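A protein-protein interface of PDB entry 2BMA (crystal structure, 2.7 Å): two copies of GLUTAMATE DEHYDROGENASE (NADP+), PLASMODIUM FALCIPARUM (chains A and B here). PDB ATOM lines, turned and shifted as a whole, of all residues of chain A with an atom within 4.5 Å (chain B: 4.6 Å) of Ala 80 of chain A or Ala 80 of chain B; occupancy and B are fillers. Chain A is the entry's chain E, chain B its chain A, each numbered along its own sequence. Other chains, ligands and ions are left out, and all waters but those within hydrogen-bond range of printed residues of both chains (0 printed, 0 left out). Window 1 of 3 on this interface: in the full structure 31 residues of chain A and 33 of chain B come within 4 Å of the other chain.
Pro 77 of chain A touches none of the printed residues of chain B.
Ala 80 of chain A touches just these residues of chain B: Ala 80 (3.6 Å), Ile 81 (3.5 Å) and Gln 82 (2.7 Å).
Printed residues of chain A within 4 Å of Arg 79 of chain B: Gln 82.
Printed residues of chain A within 4 Å of Ala 80 of chain B: Ala 80 (3.6 Å), Ile 81 (3.9 Å) and Gln 82 (2.7 Å).
Of the printed residues of chain A, Gln 82 of chain B touches Arg 79 and Ala 80.
Arg 101 of chain B touches none of the printed residues of chain A.
The nearest printed residue of chain B that does not touch Ala 80 of chain A is Arg 101 of chain B (7.3 Å).
The nearest printed residue of chain B that does not touch Arg 79 of chain A is Ile 81 of chain B (4.3 Å).
Arg 79 of chain A touches Gln 82 of chain B, and with the chains exchanged Gln 82 of chain A touches Arg 79 of chain B.
Ala 80 of chain A touches its own counterpart, Ala 80 of chain B.
Ala 80 of chain A touches Ile 81 of chain B, and with the chains exchanged Ile 81 of chain A touches Ala 80 of chain B.
Ala 80 of chain A touches Gln 82 of chain B, and with the chains exchanged Gln 82 of chain A touches Ala 80 of chain B.
Of the 7 pairs that touch across the chains among the printed residues, 7 have their exchanged pair printed and touching as well.
The backbone NH (N) of Ala 80 of chain B sits at hydrogen-bond distance from the backbone carbonyl oxygen (O) of Gln 82 of chain A (2.7 Å).
N of Ala 80 of chain A lies within hydrogen-bond range of O of Gln 82 of chain B, at 2.7 Å.
Of the 7 printed residues of chain A, 4 touch a printed residue of chain B.
Hydrophobic or aromatic side chains of chain A within 4 Å of the printed part of chain B: Ala 80.
Along chain A the printed residues that touch a printed residue of chain B span positions 79 to 82.
Hydrophobic or aromatic side chains of chain B that line the printed part of chain A: Ala 80.
Among the printed residues, 7 pairs touch across the chains.
Among the printed residues, no Asp or Glu carboxylate lies within 4 Å of a Lys or Arg side-chain nitrogen of the other chain.
O of Ile 81 of chain B is in hydrogen-bond range of N of Arg 101 of chain B (3.0 Å).
The backbone NH (N) of Ile 81 of chain A is in hydrogen-bond range of the backbone carbonyl oxygen (O) of Arg 101 of chain A.
Gln 82 of chain B touches Arg 79 of chain A.
O of Ala 80 of chain A touches O of Ala 80 of chain B, 3.6 Å away.
Ala 80 of chain A touches Ile 81 of chain B (O to CA, 3.5 Å).
Ala 80 of chain B touches Ile 81 of chain A.
Gln 82 of chain A touches Arg 79 of chain B (O to CA, 3.4 Å).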
ATOM      1  N   PRO A  77     -33.363  -4.385   9.626  1.00  0.00           N
ATOM      2  CA  PRO A  77     -34.038  -5.495  10.306  1.00  0.00           C
ATOM      3  C   PRO A  77     -33.441  -5.818  11.671  1.00  0.00           C
ATOM      4  O   PRO A  77     -32.229  -5.940  11.812  1.00  0.00           O
ATOM      5  CB  PRO A  77     -33.867  -6.653   9.327  1.00  0.00           C
ATOM      6  CG  PRO A  77     -33.840  -5.982   8.021  1.00  0.00           C
ATOM      7  CD  PRO A  77     -32.953  -4.790   8.273  1.00  0.00           C
ATOM      8  N   ARG A  79     -33.489  -8.436  12.943  1.00  0.00           N
ATOM      9  CA  ARG A  79     -32.912  -9.753  12.732  1.00  0.00           C
ATOM     10  C   ARG A  79     -33.315 -10.301  11.363  1.00  0.00           C
ATOM     11  O   ARG A  79     -34.489 -10.310  10.999  1.00  0.00           O
ATOM     12  CB  ARG A  79     -33.378 -10.689  13.850  1.00  0.00           C
ATOM     13  CG  ARG A  79     -32.764 -12.079  13.840  1.00  0.00           C
ATOM     14  CD  ARG A  79     -32.794 -12.685  15.234  1.00  0.00           C
ATOM     15  NE  ARG A  79     -34.144 -12.644  15.761  1.00  0.00           N
ATOM     16  CZ  ARG A  79     -34.463 -12.334  17.009  1.00  0.00           C
ATOM     17  NH1 ARG A  79     -33.520 -12.036  17.892  1.00  0.00           N
ATOM     18  NH2 ARG A  79     -35.738 -12.307  17.359  1.00  0.00           N
ATOM     19  N   ALA A  80     -32.320 -10.729  10.595  1.00  0.00           N
ATOM     20  CA  ALA A  80     -32.555 -11.285   9.278  1.00  0.00           C
ATOM     21  C   ALA A  80     -31.856 -12.619   9.252  1.00  0.00           C
ATOM     22  O   ALA A  80     -30.636 -12.688   9.385  1.00  0.00           O
ATOM     23  CB  ALA A  80     -31.982 -10.391   8.220  1.00  0.00           C
ATOM     24  N   ILE A  81     -32.640 -13.677   9.087  1.00  0.00           N
ATOM     25  CA  ILE A  81     -32.097 -15.027   9.048  1.00  0.00           C
ATOM     26  C   ILE A  81     -32.233 -15.669   7.670  1.00  0.00           C
ATOM     27  O   ILE A  81     -33.329 -15.771   7.119  1.00  0.00           O
ATOM     28  CB  ILE A  81     -32.800 -15.917  10.064  1.00  0.00           C
ATOM     29  CG1 ILE A  81     -32.559 -15.360  11.469  1.00  0.00           C
ATOM     30  CG2 ILE A  81     -32.310 -17.352   9.918  1.00  0.00           C
ATOM     31  CD1 ILE A  81     -33.432 -15.961  12.512  1.00  0.00           C
ATOM     32  N   GLN A  82     -31.107 -16.088   7.112  1.00  0.00           N
ATOM     33  CA  GLN A  82     -31.116 -16.725   5.811  1.00  0.00           C
ATOM     34  C   GLN A  82     -30.671 -18.150   6.075  1.00  0.00           C
ATOM     35  O   GLN A  82     -29.658 -18.354   6.751  1.00  0.00           O
ATOM     36  CB  GLN A  82     -30.153 -16.013   4.862  1.00  0.00           C
ATOM     37  CG  GLN A  82     -30.060 -16.671   3.503  1.00  0.00           C
ATOM     38  CD  GLN A  82     -29.221 -15.892   2.484  1.00  0.00           C
ATOM     39  OE1 GLN A  82     -29.608 -14.804   2.034  1.00  0.00           O
ATOM     40  NE2 GLN A  82     -28.075 -16.461   2.104  1.00  0.00           N
ATOM     41  N   ARG A 101     -36.351 -15.211   6.328  1.00  0.00           N
ATOM     42  CA  ARG A 101     -37.285 -14.867   7.373  1.00  0.00           C
ATOM     43  C   ARG A 101     -36.672 -13.661   8.043  1.00  0.00           C
ATOM     44  O   ARG A 101     -35.800 -13.778   8.908  1.00  0.00           O
ATOM     45  CB  ARG A 101     -37.479 -15.985   8.392  1.00  0.00           C
ATOM     46  CG  ARG A 101     -38.658 -15.704   9.338  1.00  0.00           C
ATOM     47  CD  ARG A 101     -39.956 -15.465   8.553  1.00  0.00           C
ATOM     48  NE  ARG A 101     -41.024 -14.880   9.365  1.00  0.00           N
ATOM     49  CZ  ARG A 101     -42.136 -14.341   8.865  1.00  0.00           C
ATOM     50  NH1 ARG A 101     -42.325 -14.316   7.555  1.00  0.00           N
ATOM     51  NH2 ARG A 101     -43.060 -13.826   9.670  1.00  0.00           N
ATOM     52  N   VAL A 102     -37.118 -12.500   7.588  1.00  0.00           N
ATOM     53  CA  VAL A 102     -36.662 -11.233   8.096  1.00  0.00           C
ATOM     54  C   VAL A 102     -37.588 -10.799   9.208  1.00  0.00           C
ATOM     55  O   VAL A 102     -38.737 -10.450   8.967  1.00  0.00           O
ATOM     56  CB  VAL A 102     -36.691 -10.183   6.986  1.00  0.00           C
ATOM     57  CG1 VAL A 102     -36.465  -8.806   7.570  1.00  0.00           C
ATOM     58  CG2 VAL A 102     -35.644 -10.511   5.936  1.00  0.00           C
ATOM     59  N   PRO B  77     -24.469 -21.202   3.199  1.00  0.00           N
ATOM     60  CA  PRO B  77     -24.447 -21.280   4.662  1.00  0.00           C
ATOM     61  C   PRO B  77     -25.674 -22.012   5.161  1.00  0.00           C
ATOM     62  O   PRO B  77     -26.778 -21.796   4.671  1.00  0.00           O
ATOM     63  CB  PRO B  77     -24.455 -19.818   5.084  1.00  0.00           C
ATOM     64  CG  PRO B  77     -23.783 -19.127   3.947  1.00  0.00           C
ATOM     65  CD  PRO B  77     -24.379 -19.802   2.748  1.00  0.00           C
ATOM     66  N   ARG B  79     -26.948 -21.559   7.849  1.00  0.00           N
ATOM     67  CA  ARG B  79     -27.689 -20.496   8.508  1.00  0.00           C
ATOM     68  C   ARG B  79     -26.823 -19.234   8.475  1.00  0.00           C
ATOM     69  O   ARG B  79     -25.611 -19.301   8.673  1.00  0.00           O
ATOM     70  CB  ARG B  79     -27.985 -20.908   9.944  1.00  0.00           C
ATOM     71  CG  ARG B  79     -29.065 -20.119  10.626  1.00  0.00           C
ATOM     72  CD  ARG B  79     -29.729 -20.985  11.673  1.00  0.00           C
ATOM     73  NE  ARG B  79     -28.739 -21.624  12.527  1.00  0.00           N
ATOM     74  CZ  ARG B  79     -28.816 -22.872  12.976  1.00  0.00           C
ATOM     75  NH1 ARG B  79     -29.847 -23.645  12.653  1.00  0.00           N
ATOM     76  NH2 ARG B  79     -27.854 -23.345  13.753  1.00  0.00           N
ATOM     77  N   ALA B  80     -27.438 -18.084   8.211  1.00  0.00           N
ATOM     78  CA  ALA B  80     -26.690 -16.836   8.148  1.00  0.00           C
ATOM     79  C   ALA B  80     -27.486 -15.710   8.786  1.00  0.00           C
ATOM     80  O   ALA B  80     -28.314 -15.086   8.129  1.00  0.00           O
ATOM     81  CB  ALA B  80     -26.388 -16.509   6.718  1.00  0.00           C
ATOM     82  N   ILE B  81     -27.215 -15.447  10.064  1.00  0.00           N
ATOM     83  CA  ILE B  81     -27.924 -14.417  10.830  1.00  0.00           C
ATOM     84  C   ILE B  81     -27.303 -13.029  10.769  1.00  0.00           C
ATOM     85  O   ILE B  81     -26.141 -12.851  11.095  1.00  0.00           O
ATOM     86  CB  ILE B  81     -28.015 -14.815  12.312  1.00  0.00           C
ATOM     87  CG1 ILE B  81     -28.505 -16.256  12.417  1.00  0.00           C
ATOM     88  CG2 ILE B  81     -28.948 -13.856  13.070  1.00  0.00           C
ATOM     89  CD1 ILE B  81     -27.770 -17.086  13.447  1.00  0.00           C
ATOM     90  N   GLN B  82     -28.107 -12.059  10.347  1.00  0.00           N
ATOM     91  CA  GLN B  82     -27.711 -10.658  10.238  1.00  0.00           C
ATOM     92  C   GLN B  82     -28.592  -9.960  11.259  1.00  0.00           C
ATOM     93  O   GLN B  82     -29.774 -10.279  11.373  1.00  0.00           O
ATOM     94  CB  GLN B  82     -28.015 -10.119   8.830  1.00  0.00           C
ATOM     95  CG  GLN B  82     -27.716  -8.638   8.634  1.00  0.00           C
ATOM     96  CD  GLN B  82     -27.882  -8.173   7.189  1.00  0.00           C
ATOM     97  OE1 GLN B  82     -27.223  -8.677   6.276  1.00  0.00           O
ATOM     98  NE2 GLN B  82     -28.764  -7.201   6.980  1.00  0.00           N
ATOM     99  N   ARG B 101     -23.294 -13.414  11.722  1.00  0.00           N
ATOM    100  CA  ARG B 101     -22.880 -14.684  12.270  1.00  0.00           C
ATOM    101  C   ARG B 101     -23.316 -15.706  11.266  1.00  0.00           C
ATOM    102  O   ARG B 101     -24.467 -16.140  11.266  1.00  0.00           O
ATOM    103  CB  ARG B 101     -23.514 -15.005  13.618  1.00  0.00           C
ATOM    104  CG  ARG B 101     -22.809 -16.190  14.286  1.00  0.00           C
ATOM    105  CD  ARG B 101     -21.295 -15.950  14.284  1.00  0.00           C
ATOM    106  NE  ARG B 101     -20.486 -17.119  14.627  1.00  0.00           N
ATOM    107  CZ  ARG B 101     -19.154 -17.139  14.574  1.00  0.00           C
ATOM    108  NH1 ARG B 101     -18.498 -16.062  14.191  1.00  0.00           N
ATOM    109  NH2 ARG B 101     -18.474 -18.223  14.904  1.00  0.00           N
ATOM    110  N   VAL B 102     -22.394 -16.061  10.379  1.00  0.00           N
ATOM    111  CA  VAL B 102     -22.675 -17.043   9.356  1.00  0.00           C
ATOM    112  C   VAL B 102     -22.274 -18.421   9.840  1.00  0.00           C
ATOM    113  O   VAL B 102     -21.090 -18.720   9.949  1.00  0.00           O
ATOM    114  CB  VAL B 102     -21.906 -16.732   8.075  1.00  0.00           C
ATOM    115  CG1 VAL B 102     -22.034 -17.890   7.110  1.00  0.00           C
ATOM    116  CG2 VAL B 102     -22.435 -15.454   7.453  1.00  0.00           C
